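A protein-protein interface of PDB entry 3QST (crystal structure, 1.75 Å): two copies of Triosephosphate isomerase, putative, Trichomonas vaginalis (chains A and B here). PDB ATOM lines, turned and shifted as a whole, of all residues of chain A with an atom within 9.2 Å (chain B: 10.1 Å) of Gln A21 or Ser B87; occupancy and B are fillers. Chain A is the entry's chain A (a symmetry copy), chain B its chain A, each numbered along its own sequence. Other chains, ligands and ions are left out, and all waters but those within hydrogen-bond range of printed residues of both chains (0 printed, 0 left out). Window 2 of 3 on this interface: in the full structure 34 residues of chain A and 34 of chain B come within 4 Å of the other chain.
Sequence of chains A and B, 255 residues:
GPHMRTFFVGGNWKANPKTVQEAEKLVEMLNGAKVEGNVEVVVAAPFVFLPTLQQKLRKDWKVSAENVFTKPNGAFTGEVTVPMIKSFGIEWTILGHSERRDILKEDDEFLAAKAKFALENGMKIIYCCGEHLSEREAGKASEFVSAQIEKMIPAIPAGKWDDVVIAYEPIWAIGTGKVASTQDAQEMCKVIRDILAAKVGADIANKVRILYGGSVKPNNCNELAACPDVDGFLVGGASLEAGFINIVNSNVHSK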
ATOM      1  N   TRP A  13     -23.837 -19.444 -12.086  1.00  0.00           N
ATOM      2  CA  TRP A  13     -22.810 -18.412 -12.175  1.00  0.00           C
ATOM      3  C   TRP A  13     -22.956 -17.534 -13.417  1.00  0.00           C
ATOM      4  O   TRP A  13     -22.351 -16.460 -13.480  1.00  0.00           O
ATOM      5  CB  TRP A  13     -21.425 -19.028 -12.223  1.00  0.00           C
ATOM      6  CG  TRP A  13     -21.012 -19.702 -10.979  1.00  0.00           C
ATOM      7  CD1 TRP A  13     -21.781 -19.968  -9.871  1.00  0.00           C
ATOM      8  CD2 TRP A  13     -19.708 -20.198 -10.696  1.00  0.00           C
ATOM      9  NE1 TRP A  13     -21.013 -20.605  -8.914  1.00  0.00           N
ATOM     10  CE2 TRP A  13     -19.741 -20.758  -9.403  1.00  0.00           C
ATOM     11  CE3 TRP A  13     -18.507 -20.228 -11.422  1.00  0.00           C
ATOM     12  CZ2 TRP A  13     -18.615 -21.339  -8.817  1.00  0.00           C
ATOM     13  CZ3 TRP A  13     -17.398 -20.800 -10.837  1.00  0.00           C
ATOM     14  CH2 TRP A  13     -17.460 -21.345  -9.546  1.00  0.00           C
ATOM     15  N   PRO A  17     -17.009 -16.381 -13.054  1.00  0.00           N
ATOM     16  CA  PRO A  17     -16.273 -15.116 -12.982  1.00  0.00           C
ATOM     17  C   PRO A  17     -15.400 -14.946 -14.226  1.00  0.00           C
ATOM     18  O   PRO A  17     -15.496 -15.740 -15.148  1.00  0.00           O
ATOM     19  CB  PRO A  17     -15.402 -15.293 -11.736  1.00  0.00           C
ATOM     20  CG  PRO A  17     -15.129 -16.751 -11.679  1.00  0.00           C
ATOM     21  CD  PRO A  17     -16.401 -17.423 -12.210  1.00  0.00           C
ATOM     22  N   LYS A  18     -14.574 -13.906 -14.256  1.00  0.00           N
ATOM     23  CA  LYS A  18     -13.731 -13.643 -15.418  1.00  0.00           C
ATOM     24  C   LYS A  18     -12.584 -14.637 -15.590  1.00  0.00           C
ATOM     25  O   LYS A  18     -12.146 -14.893 -16.715  1.00  0.00           O
ATOM     26  CB  LYS A  18     -13.187 -12.210 -15.370  1.00  0.00           C
ATOM     27  CG  LYS A  18     -14.224 -11.155 -15.761  1.00  0.00           C
ATOM     28  CD  LYS A  18     -13.613  -9.753 -15.804  1.00  0.00           C
ATOM     29  CE  LYS A  18     -12.908  -9.407 -14.507  1.00  0.00           C
ATOM     30  NZ  LYS A  18     -13.860  -9.128 -13.395  1.00  0.00           N
ATOM     31  N   THR A  19     -12.104 -15.220 -14.494  1.00  0.00           N
ATOM     32  CA  THR A  19     -10.901 -16.046 -14.568  1.00  0.00           C
ATOM     33  C   THR A  19     -11.009 -17.394 -13.860  1.00  0.00           C
ATOM     34  O   THR A  19     -11.759 -17.562 -12.890  1.00  0.00           O
ATOM     35  CB  THR A  19      -9.669 -15.314 -13.984  1.00  0.00           C
ATOM     36  OG1 THR A  19      -9.828 -15.157 -12.560  1.00  0.00           O
ATOM     37  CG2 THR A  19      -9.490 -13.938 -14.647  1.00  0.00           C
ATOM     38  N   VAL A  20     -10.227 -18.353 -14.332  1.00  0.00           N
ATOM     39  CA  VAL A  20     -10.217 -19.657 -13.696  1.00  0.00           C
ATOM     40  C   VAL A  20      -9.692 -19.547 -12.255  1.00  0.00           C
ATOM     41  O   VAL A  20     -10.104 -20.301 -11.366  1.00  0.00           O
ATOM     42  CB  VAL A  20      -9.417 -20.685 -14.515  1.00  0.00           C
ATOM     43  CG1 VAL A  20      -7.916 -20.300 -14.573  1.00  0.00           C
ATOM     44  CG2 VAL A  20      -9.624 -22.104 -13.938  1.00  0.00           C
ATOM     45  N   GLN A  21      -8.806 -18.588 -12.019  1.00  0.00           N
ATOM     46  CA  GLN A  21      -8.278 -18.398 -10.673  1.00  0.00           C
ATOM     47  C   GLN A  21      -9.389 -17.964  -9.711  1.00  0.00           C
ATOM     48  O   GLN A  21      -9.464 -18.454  -8.578  1.00  0.00           O
ATOM     49  CB  GLN A  21      -7.111 -17.412 -10.691  1.00  0.00           C
ATOM     50  CG  GLN A  21      -5.913 -17.938 -11.486  1.00  0.00           C
ATOM     51  CD  GLN A  21      -6.041 -17.704 -12.989  1.00  0.00           C
ATOM     52  OE1 GLN A  21      -6.933 -16.993 -13.442  1.00  0.00           O
ATOM     53  NE2 GLN A  21      -5.140 -18.296 -13.763  1.00  0.00           N
ATOM     54  N   GLU A  22     -10.268 -17.069 -10.170  1.00  0.00           N
ATOM     55  CA  GLU A  22     -11.438 -16.689  -9.381  1.00  0.00           C
ATOM     56  C   GLU A  22     -12.412 -17.853  -9.193  1.00  0.00           C
ATOM     57  O   GLU A  22     -12.997 -18.004  -8.116  1.00  0.00           O
ATOM     58  CB  GLU A  22     -12.187 -15.523 -10.020  1.00  0.00           C
ATOM     59  CG  GLU A  22     -11.505 -14.175  -9.919  1.00  0.00           C
ATOM     60  CD  GLU A  22     -12.123 -13.189 -10.891  1.00  0.00           C
ATOM     61  OE1 GLU A  22     -11.764 -13.224 -12.090  1.00  0.00           O
ATOM     62  OE2 GLU A  22     -12.987 -12.395 -10.466  1.00  0.00           O
ATOM     63  N   ALA A  23     -12.632 -18.635 -10.252  1.00  0.00           N
ATOM     64  CA  ALA A  23     -13.504 -19.811 -10.157  1.00  0.00           C
ATOM     65  C   ALA A  23     -12.998 -20.757  -9.067  1.00  0.00           C
ATOM     66  O   ALA A  23     -13.771 -21.275  -8.263  1.00  0.00           O
ATOM     67  CB  ALA A  23     -13.569 -20.532 -11.495  1.00  0.00           C
ATOM     68  N   GLU A  24     -11.690 -20.979  -9.042  1.00  0.00           N
ATOM     69  CA  GLU A  24     -11.096 -21.851  -8.025  1.00  0.00           C
ATOM     70  C   GLU A  24     -11.272 -21.310  -6.595  1.00  0.00           C
ATOM     71  O   GLU A  24     -11.544 -22.081  -5.666  1.00  0.00           O
ATOM     72  CB  GLU A  24      -9.624 -22.146  -8.369  1.00  0.00           C
ATOM     73  CG  GLU A  24      -9.571 -23.162  -9.510  1.00  0.00           C
ATOM     74  CD  GLU A  24      -8.201 -23.416 -10.087  1.00  0.00           C
ATOM     75  OE1 GLU A  24      -7.233 -22.750  -9.679  1.00  0.00           O
ATOM     76  OE2 GLU A  24      -8.121 -24.285 -10.983  1.00  0.00           O
ATOM     77  N   LYS A  25     -11.134 -20.003  -6.423  1.00  0.00           N
ATOM     78  CA  LYS A  25     -11.359 -19.369  -5.117  1.00  0.00           C
ATOM     79  C   LYS A  25     -12.817 -19.533  -4.662  1.00  0.00           C
ATOM     80  O   LYS A  25     -13.082 -19.795  -3.483  1.00  0.00           O
ATOM     81  CB  LYS A  25     -10.968 -17.888  -5.153  1.00  0.00           C
ATOM     82  N   LEU A  26     -13.758 -19.393  -5.600  1.00  0.00           N
ATOM     83  CA  LEU A  26     -15.184 -19.601  -5.295  1.00  0.00           C
ATOM     84  C   LEU A  26     -15.475 -21.031  -4.839  1.00  0.00           C
ATOM     85  O   LEU A  26     -16.233 -21.255  -3.891  1.00  0.00           O
ATOM     86  CB  LEU A  26     -16.061 -19.270  -6.502  1.00  0.00           C
ATOM     87  CG  LEU A  26     -16.121 -17.806  -6.919  1.00  0.00           C
ATOM     88  CD1 LEU A  26     -16.812 -17.669  -8.283  1.00  0.00           C
ATOM     89  CD2 LEU A  26     -16.835 -16.991  -5.856  1.00  0.00           C
ATOM     90  N   VAL A  27     -14.894 -21.998  -5.538  1.00  0.00           N
ATOM     91  CA  VAL A  27     -15.055 -23.399  -5.170  1.00  0.00           C
ATOM     92  C   VAL A  27     -14.502 -23.634  -3.752  1.00  0.00           C
ATOM     93  O   VAL A  27     -15.120 -24.322  -2.949  1.00  0.00           O
ATOM     94  CB  VAL A  27     -14.359 -24.322  -6.180  1.00  0.00           C
ATOM     95  CG1 VAL A  27     -14.278 -25.743  -5.661  1.00  0.00           C
ATOM     96  CG2 VAL A  27     -15.113 -24.289  -7.509  1.00  0.00           C
ATOM     97  N   GLU A  28     -13.355 -23.043  -3.446  1.00  0.00           N
ATOM     98  CA  GLU A  28     -12.795 -23.202  -2.096  1.00  0.00           C
ATOM     99  C   GLU A  28     -13.766 -22.676  -1.032  1.00  0.00           C
ATOM    100  O   GLU A  28     -13.954 -23.309   0.008  1.00  0.00           O
ATOM    101  CB  GLU A  28     -11.421 -22.535  -1.979  1.00  0.00           C
ATOM    102  CG  GLU A  28     -10.333 -23.290  -2.727  1.00  0.00           C
ATOM    103  CD  GLU A  28     -10.306 -24.777  -2.375  1.00  0.00           C
ATOM    104  OE1 GLU A  28     -10.123 -25.091  -1.180  1.00  0.00           O
ATOM    105  OE2 GLU A  28     -10.480 -25.631  -3.285  1.00  0.00           O
ATOM    106  N   VAL A  48     -15.594 -23.514 -19.787  1.00  0.00           N
ATOM    107  CA  VAL A  48     -14.146 -23.656 -19.605  1.00  0.00           C
ATOM    108  C   VAL A  48     -13.741 -23.883 -18.158  1.00  0.00           C
ATOM    109  O   VAL A  48     -12.607 -24.303 -17.880  1.00  0.00           O
ATOM    110  CB  VAL A  48     -13.336 -22.485 -20.199  1.00  0.00           C
ATOM    111  CG1 VAL A  48     -13.439 -22.500 -21.727  1.00  0.00           C
ATOM    112  CG2 VAL A  48     -13.760 -21.129 -19.584  1.00  0.00           C
ATOM    113  N   PHE A  49     -14.675 -23.627 -17.240  1.00  0.00           N
ATOM    114  CA  PHE A  49     -14.427 -23.846 -15.820  1.00  0.00           C
ATOM    115  C   PHE A  49     -15.009 -25.171 -15.328  1.00  0.00           C
ATOM    116  O   PHE A  49     -14.817 -25.538 -14.168  1.00  0.00           O
ATOM    117  CB  PHE A  49     -15.020 -22.710 -14.965  1.00  0.00           C
ATOM    118  CG  PHE A  49     -14.465 -21.341 -15.271  1.00  0.00           C
ATOM    119  CD1 PHE A  49     -13.190 -21.181 -15.813  1.00  0.00           C
ATOM    120  CD2 PHE A  49     -15.223 -20.203 -15.005  1.00  0.00           C
ATOM    121  CE1 PHE A  49     -12.701 -19.915 -16.096  1.00  0.00           C
ATOM    122  CE2 PHE A  49     -14.730 -18.930 -15.281  1.00  0.00           C
ATOM    123  CZ  PHE A  49     -13.465 -18.787 -15.822  1.00  0.00           C
ATOM    124  N   THR A  52     -12.462 -27.860 -13.921  1.00  0.00           N
ATOM    125  CA  THR A  52     -11.879 -27.599 -12.618  1.00  0.00           C
ATOM    126  C   THR A  52     -12.939 -27.717 -11.515  1.00  0.00           C
ATOM    127  O   THR A  52     -12.656 -28.232 -10.431  1.00  0.00           O
ATOM    128  CB  THR A  52     -11.063 -26.284 -12.570  1.00  0.00           C
ATOM    129  OG1 THR A  52     -10.201 -26.310 -11.422  1.00  0.00           O
ATOM    130  CG2 THR A  52     -11.958 -25.076 -12.516  1.00  0.00           C
ATOM    131  N   LEU A  53     -14.170 -27.291 -11.798  1.00  0.00           N
ATOM    132  CA  LEU A  53     -15.252 -27.510 -10.833  1.00  0.00           C
ATOM    133  C   LEU A  53     -15.477 -28.993 -10.559  1.00  0.00           C
ATOM    134  O   LEU A  53     -15.633 -29.406  -9.411  1.00  0.00           O
ATOM    135  CB  LEU A  53     -16.560 -26.851 -11.295  1.00  0.00           C
ATOM    136  CG  LEU A  53     -16.861 -25.499 -10.649  1.00  0.00           C
ATOM    137  CD1 LEU A  53     -15.845 -24.451 -11.088  1.00  0.00           C
ATOM    138  CD2 LEU A  53     -18.286 -25.055 -10.999  1.00  0.00           C
ATOM    139  N   LYS A  56     -12.654 -30.238  -8.366  1.00  0.00           N
ATOM    140  CA  LYS A  56     -12.402 -29.586  -7.077  1.00  0.00           C
ATOM    141  C   LYS A  56     -13.619 -29.377  -6.167  1.00  0.00           C
ATOM    142  O   LYS A  56     -13.462 -29.235  -4.956  1.00  0.00           O
ATOM    143  CB  LYS A  56     -11.691 -28.245  -7.296  1.00  0.00           C
ATOM    144  CG  LYS A  56     -10.311 -28.392  -7.938  1.00  0.00           C
ATOM    145  CD  LYS A  56      -9.613 -27.053  -8.088  1.00  0.00           C
ATOM    146  CE  LYS A  56      -8.208 -27.245  -8.655  1.00  0.00           C
ATOM    147  NZ  LYS A  56      -8.274 -27.818 -10.034  1.00  0.00           N
ATOM    148  N   LEU B  50     -10.574 -27.143 -23.800  1.00  0.00           N
ATOM    149  CA  LEU B  50      -9.526 -26.144 -23.935  1.00  0.00           C
ATOM    150  C   LEU B  50      -8.500 -26.226 -22.794  1.00  0.00           C
ATOM    151  O   LEU B  50      -7.301 -26.115 -23.033  1.00  0.00           O
ATOM    152  CB  LEU B  50     -10.113 -24.730 -24.066  1.00  0.00           C
ATOM    153  CG  LEU B  50     -10.890 -24.416 -25.358  1.00  0.00           C
ATOM    154  CD1 LEU B  50     -11.444 -23.004 -25.278  1.00  0.00           C
ATOM    155  CD2 LEU B  50     -10.004 -24.572 -26.619  1.00  0.00           C
ATOM    156  N   PRO B  51      -8.964 -26.446 -21.554  1.00  0.00           N
ATOM    157  CA  PRO B  51      -7.932 -26.527 -20.518  1.00  0.00           C
ATOM    158  C   PRO B  51      -6.953 -27.673 -20.737  1.00  0.00           C
ATOM    159  O   PRO B  51      -5.740 -27.499 -20.560  1.00  0.00           O
ATOM    160  CB  PRO B  51      -8.748 -26.700 -19.228  1.00  0.00           C
ATOM    161  CG  PRO B  51     -10.047 -26.002 -19.546  1.00  0.00           C
ATOM    162  CD  PRO B  51     -10.324 -26.391 -20.973  1.00  0.00           C
ATOM    163  N   GLN B  54      -4.557 -26.805 -23.551  1.00  0.00           N
ATOM    164  CA  GLN B  54      -3.584 -25.789 -23.161  1.00  0.00           C
ATOM    165  C   GLN B  54      -2.473 -26.412 -22.326  1.00  0.00           C
ATOM    166  O   GLN B  54      -1.292 -26.071 -22.484  1.00  0.00           O
ATOM    167  CB  GLN B  54      -4.267 -24.669 -22.374  1.00  0.00           C
ATOM    168  CG  GLN B  54      -3.325 -23.540 -21.958  1.00  0.00           C
ATOM    169  CD  GLN B  54      -2.721 -22.803 -23.150  1.00  0.00           C
ATOM    170  OE1 GLN B  54      -3.190 -22.935 -24.285  1.00  0.00           O
ATOM    171  NE2 GLN B  54      -1.680 -22.017 -22.891  1.00  0.00           N
ATOM    172  N   PRO B  72     -17.049  -8.889 -21.251  1.00  0.00           N
ATOM    173  CA  PRO B  72     -16.051  -9.569 -20.412  1.00  0.00           C
ATOM    174  C   PRO B  72     -16.635 -10.670 -19.520  1.00  0.00           C
ATOM    175  O   PRO B  72     -15.951 -11.643 -19.205  1.00  0.00           O
ATOM    176  CB  PRO B  72     -15.484  -8.437 -19.547  1.00  0.00           C
ATOM    177  CG  PRO B  72     -16.521  -7.389 -19.552  1.00  0.00           C
ATOM    178  CD  PRO B  72     -17.207  -7.467 -20.892  1.00  0.00           C
ATOM    179  N   VAL B  80     -19.165 -18.154 -23.148  1.00  0.00           N
ATOM    180  CA  VAL B  80     -17.784 -18.046 -22.665  1.00  0.00           C
ATOM    181  C   VAL B  80     -17.152 -16.745 -23.153  1.00  0.00           C
ATOM    182  O   VAL B  80     -17.373 -16.332 -24.291  1.00  0.00           O
ATOM    183  CB  VAL B  80     -16.931 -19.246 -23.151  1.00  0.00           C
ATOM    184  CG1 VAL B  80     -15.442 -19.052 -22.822  1.00  0.00           C
ATOM    185  CG2 VAL B  80     -17.456 -20.555 -22.539  1.00  0.00           C
ATOM    186  N   THR B  81     -16.387 -16.084 -22.288  1.00  0.00           N
ATOM    187  CA  THR B  81     -15.858 -14.761 -22.629  1.00  0.00           C
ATOM    188  C   THR B  81     -14.339 -14.761 -22.775  1.00  0.00           C
ATOM    189  O   THR B  81     -13.655 -15.686 -22.342  1.00  0.00           O
ATOM    190  CB  THR B  81     -16.275 -13.709 -21.589  1.00  0.00           C
ATOM    191  OG1 THR B  81     -15.630 -14.006 -20.352  1.00  0.00           O
ATOM    192  CG2 THR B  81     -17.809 -13.717 -21.390  1.00  0.00           C
ATOM    193  N   VAL B  82     -13.830 -13.713 -23.410  1.00  0.00           N
ATOM    194  CA  VAL B  82     -12.395 -13.544 -23.640  1.00  0.00           C
ATOM    195  C   VAL B  82     -11.552 -13.642 -22.361  1.00  0.00           C
ATOM    196  O   VAL B  82     -10.548 -14.363 -22.333  1.00  0.00           O
ATOM    197  CB  VAL B  82     -12.122 -12.218 -24.405  1.00  0.00           C
ATOM    198  CG1 VAL B  82     -10.645 -11.851 -24.383  1.00  0.00           C
ATOM    199  CG2 VAL B  82     -12.625 -12.340 -25.841  1.00  0.00           C
ATOM    200  N   PRO B  83     -11.940 -12.921 -21.294  1.00  0.00           N
ATOM    201  CA  PRO B  83     -11.108 -13.043 -20.090  1.00  0.00           C
ATOM    202  C   PRO B  83     -11.000 -14.487 -19.583  1.00  0.00           C
ATOM    203  O   PRO B  83      -9.964 -14.882 -19.041  1.00  0.00           O
ATOM    204  CB  PRO B  83     -11.848 -12.164 -19.069  1.00  0.00           C
ATOM    205  CG  PRO B  83     -12.518 -11.120 -19.919  1.00  0.00           C
ATOM    206  CD  PRO B  83     -12.948 -11.850 -21.166  1.00  0.00           C
ATOM    207  N   MET B  84     -12.060 -15.267 -19.751  1.00  0.00           N
ATOM    208  CA  MET B  84     -12.049 -16.640 -19.244  1.00  0.00           C
ATOM    209  C   MET B  84     -11.013 -17.472 -20.000  1.00  0.00           C
ATOM    210  O   MET B  84     -10.236 -18.216 -19.406  1.00  0.00           O
ATOM    211  CB  MET B  84     -13.424 -17.291 -19.409  1.00  0.00           C
ATOM    212  CG  MET B  84     -14.554 -16.596 -18.659  1.00  0.00           C
ATOM    213  SD  MET B  84     -16.095 -17.436 -19.077  1.00  0.00           S
ATOM    214  CE  MET B  84     -17.327 -16.354 -18.348  1.00  0.00           C
ATOM    215  N   ILE B  85     -11.056 -17.372 -21.325  1.00  0.00           N
ATOM    216  CA  ILE B  85     -10.077 -18.006 -22.197  1.00  0.00           C
ATOM    217  C   ILE B  85      -8.639 -17.569 -21.872  1.00  0.00           C
ATOM    218  O   ILE B  85      -7.726 -18.405 -21.740  1.00  0.00           O
ATOM    219  CB  ILE B  85     -10.399 -17.648 -23.677  1.00  0.00           C
ATOM    220  CG1 ILE B  85     -11.792 -18.165 -24.033  1.00  0.00           C
ATOM    221  CG2 ILE B  85      -9.370 -18.229 -24.622  1.00  0.00           C
ATOM    222  CD1 ILE B  85     -11.945 -19.606 -23.759  1.00  0.00           C
ATOM    223  N   LYS B  86      -8.435 -16.262 -21.755  1.00  0.00           N
ATOM    224  CA  LYS B  86      -7.100 -15.729 -21.484  1.00  0.00           C
ATOM    225  C   LYS B  86      -6.553 -16.172 -20.144  1.00  0.00           C
ATOM    226  O   LYS B  86      -5.334 -16.227 -19.964  1.00  0.00           O
ATOM    227  CB  LYS B  86      -7.106 -14.206 -21.523  1.00  0.00           C
ATOM    228  CG  LYS B  86      -7.470 -13.643 -22.888  1.00  0.00           C
ATOM    229  CD  LYS B  86      -7.324 -12.132 -22.918  1.00  0.00           C
ATOM    230  CE  LYS B  86      -5.881 -11.714 -22.663  1.00  0.00           C
ATOM    231  NZ  LYS B  86      -4.973 -12.328 -23.666  1.00  0.00           N
ATOM    232  N   SER B  87      -7.443 -16.467 -19.200  1.00  0.00           N
ATOM    233  CA  SER B  87      -6.996 -16.865 -17.865  1.00  0.00           C
ATOM    234  C   SER B  87      -6.280 -18.223 -17.894  1.00  0.00           C
ATOM    235  O   SER B  87      -5.582 -18.590 -16.942  1.00  0.00           O
ATOM    236  CB  SER B  87      -8.168 -16.851 -16.868  1.00  0.00           C
ATOM    237  OG  SER B  87      -9.041 -17.961 -17.056  1.00  0.00           O
ATOM    238  N   PHE B  88      -6.443 -18.957 -18.995  1.00  0.00           N
ATOM    239  CA  PHE B  88      -5.736 -20.223 -19.193  1.00  0.00           C
ATOM    240  C   PHE B  88      -4.462 -20.034 -20.011  1.00  0.00           C
ATOM    241  O   PHE B  88      -3.661 -20.964 -20.142  1.00  0.00           O
ATOM    242  CB  PHE B  88      -6.624 -21.247 -19.911  1.00  0.00           C
ATOM    243  CG  PHE B  88      -7.740 -21.792 -19.052  1.00  0.00           C
ATOM    244  CD1 PHE B  88      -7.514 -22.853 -18.189  1.00  0.00           C
ATOM    245  CD2 PHE B  88      -9.008 -21.232 -19.101  1.00  0.00           C
ATOM    246  CE1 PHE B  88      -8.534 -23.354 -17.394  1.00  0.00           C
ATOM    247  CE2 PHE B  88     -10.036 -21.727 -18.311  1.00  0.00           C
ATOM    248  CZ  PHE B  88      -9.796 -22.786 -17.454  1.00  0.00           C
ATOM    249  N   GLY B  89      -4.289 -18.841 -20.560  1.00  0.00           N
ATOM    250  CA  GLY B  89      -3.137 -18.549 -21.407  1.00  0.00           C
ATOM    251  C   GLY B  89      -3.426 -18.773 -22.881  1.00  0.00           C
ATOM    252  O   GLY B  89      -2.523 -18.752 -23.716  1.00  0.00           O
ATOM    253  N   ILE B  90      -4.698 -18.981 -23.202  1.00  0.00           N
ATOM    254  CA  ILE B  90      -5.126 -19.186 -24.590  1.00  0.00           C
ATOM    255  C   ILE B  90      -5.217 -17.844 -25.324  1.00  0.00           C
ATOM    256  O   ILE B  90      -5.800 -16.883 -24.802  1.00  0.00           O
ATOM    257  CB  ILE B  90      -6.472 -19.913 -24.625  1.00  0.00           C
ATOM    258  CG1 ILE B  90      -6.308 -21.331 -24.066  1.00  0.00           C
ATOM    259  CG2 ILE B  90      -7.014 -19.970 -26.051  1.00  0.00           C
ATOM    260  CD1 ILE B  90      -7.589 -21.977 -23.661  1.00  0.00           C
ATOM    261  N   GLU B  91      -4.658 -17.798 -26.541  1.00  0.00           N
ATOM    262  CA  GLU B  91      -4.387 -16.543 -27.238  1.00  0.00           C
ATOM    263  C   GLU B  91      -5.277 -16.307 -28.470  1.00  0.00           C
ATOM    264  O   GLU B  91      -5.324 -15.200 -28.992  1.00  0.00           O
ATOM    265  CB  GLU B  91      -2.912 -16.515 -27.694  1.00  0.00           C
ATOM    266  CG  GLU B  91      -1.898 -16.647 -26.553  1.00  0.00           C
ATOM    267  CD  GLU B  91      -0.478 -16.866 -27.048  1.00  0.00           C
ATOM    268  OE1 GLU B  91       0.303 -17.523 -26.328  1.00  0.00           O
ATOM    269  OE2 GLU B  91      -0.150 -16.382 -28.154  1.00  0.00           O
ATOM    270  N   TRP B  92      -5.970 -17.352 -28.918  1.00  0.00           N
ATOM    271  CA  TRP B  92      -6.690 -17.316 -30.200  1.00  0.00           C
ATOM    272  C   TRP B  92      -8.168 -17.618 -30.069  1.00  0.00           C
ATOM    273  O   TRP B  92      -8.574 -18.403 -29.222  1.00  0.00           O
ATOM    274  CB  TRP B  92      -6.121 -18.400 -31.130  1.00  0.00           C
ATOM    275  CG  TRP B  92      -4.834 -18.040 -31.794  1.00  0.00           C
ATOM    276  CD1 TRP B  92      -3.574 -18.342 -31.359  1.00  0.00           C
ATOM    277  CD2 TRP B  92      -4.673 -17.307 -33.020  1.00  0.00           C
ATOM    278  NE1 TRP B  92      -2.641 -17.850 -32.239  1.00  0.00           N
ATOM    279  CE2 TRP B  92      -3.286 -17.207 -33.266  1.00  0.00           C
ATOM    280  CE3 TRP B  92      -5.565 -16.723 -33.927  1.00  0.00           C
ATOM    281  CZ2 TRP B  92      -2.760 -16.545 -34.391  1.00  0.00           C
ATOM    282  CZ3 TRP B  92      -5.047 -16.066 -35.044  1.00  0.00           C
ATOM    283  CH2 TRP B  92      -3.657 -15.979 -35.261  1.00  0.00           C
ATOM    284  N   ASN B 121      -8.772  -6.773 -26.268  1.00  0.00           N
ATOM    285  CA  ASN B 121      -8.388  -7.501 -25.064  1.00  0.00           C
ATOM    286  C   ASN B 121      -7.250  -8.481 -25.288  1.00  0.00           C
ATOM    287  O   ASN B 121      -7.039  -9.414 -24.508  1.00  0.00           O
ATOM    288  CB  ASN B 121      -9.605  -8.177 -24.442  1.00  0.00           C
ATOM    289  CG  ASN B 121     -10.480  -7.185 -23.711  1.00  0.00           C
ATOM    290  OD1 ASN B 121     -10.265  -6.923 -22.529  1.00  0.00           O
ATOM    291  ND2 ASN B 121     -11.436  -6.587 -24.418  1.00  0.00           N
ATOM    292  N   MET B 123      -6.517 -10.643 -27.772  1.00  0.00           N
ATOM    293  CA  MET B 123      -6.656 -11.901 -28.519  1.00  0.00           C
ATOM    294  C   MET B 123      -6.188 -11.752 -29.961  1.00  0.00           C
ATOM    295  O   MET B 123      -6.135 -10.645 -30.510  1.00  0.00           O
ATOM    296  CB  MET B 123      -8.117 -12.341 -28.583  1.00  0.00           C
ATOM    297  CG  MET B 123      -8.778 -12.491 -27.265  1.00  0.00           C
ATOM    298  SD  MET B 123      -8.079 -13.917 -26.455  1.00  0.00           S
ATOM    299  CE  MET B 123      -8.531 -15.222 -27.610  1.00  0.00           C
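No position is printed for both chains.
Along chain A the printed residues that touch a printed residue of chain B span positions 17 to 49.
Hydrophobic or aromatic side chains of chain B that line the printed part of chain A: Pro B51, Pro B83, Met B84, Ile B85 and Phe B88.
Among the printed residues, 14 pairs touch across the chains.
Among the printed residues, no Asp or Glu carboxylate lies within 4 Å of a Lys or Arg side-chain nitrogen of the other chain.
The side-chain hydroxyl of Thr A19 sits at hydrogen-bond distance from the side-chain carboxylate of Glu A22 (2.8 Å).
The backbone carbonyl oxygen of Pro B72 is in hydrogen-bond range of the side-chain hydroxyl of Thr B81 (2.6 Å).
The side-chain hydroxyl (OG) of Ser B87 sits at hydrogen-bond distance from the backbone carbonyl oxygen (O) of Met B84, at 2.6 Å.
N of Thr B81 sits at hydrogen-bond distance from SD of Met B84.
The backbone carbonyl oxygen of Ile B85 lies within hydrogen-bond range of the backbone NH of Ile B90 (3.4 Å).
Met B84 touches Pro A17.
Pro B72 touches Lys A18.
Thr A19 touches Ser B87 (CB to CB, 3.6 Å).
Phe B88 touches Val A20.
Val A48 touches Pro B51.
Val A48 touches Met B84 (CG2 to CB, 3.9 Å).
CG1 of Val A48 touches CD1 of Ile B85, 3.8 Å away.
Val A48 touches Phe B88 (O to CZ, 3.2 Å).
Met B84 touches Phe A49.
CE1 of Phe A49 touches CE2 of Phe B88 (3.9 Å).
N of Met B84 lies within hydrogen-bond range of O of Lys A18, 3.1 Å away.
NE2 of Gln A21 lies within hydrogen-bond range of O of Ser B87, at 3.2 Å.
The backbone carbonyl oxygen (O) of Pro B83 lies close to the backbone carbonyl oxygen (O) of Lys A18 (3.2 Å).
The backbone NH (N) of Val A20 is in hydrogen-bond range of the side-chain hydroxyl (OG) of Ser B87, at 3.0 Å.
Printed residues of chain B within 4 Å of Gln A21: Ser B87.
Of the printed residues of chain A, Ser B87 touches Thr A19 (3.6 Å), Val A20 (3.0 Å) and Gln A21 (3.2 Å).
Of chain B, only Ser B87 (3.6 Å) comes within 4 Å of Thr A19.
Of chain B, only Ser B87 and Phe B88 come within 4 Å of Val A20.
No residue of chain B comes within 4 Å of Ala A23.
No residue of chain B comes within 4 Å of Glu A24.
Of the printed residues of chain B, Phe A49 touches Met B84 (3.7 Å) and Phe B88 (3.9 Å).
Printed residues of chain B within 4 Å of Pro A17: Met B84 (3.7 Å).
Printed residues of chain B within 4 Å of Val A48: Pro B51, Met B84, Ile B85 and Phe B88.
Printed residues of chain A within 4 Å of Pro B83: Lys A18 (3.1 Å).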
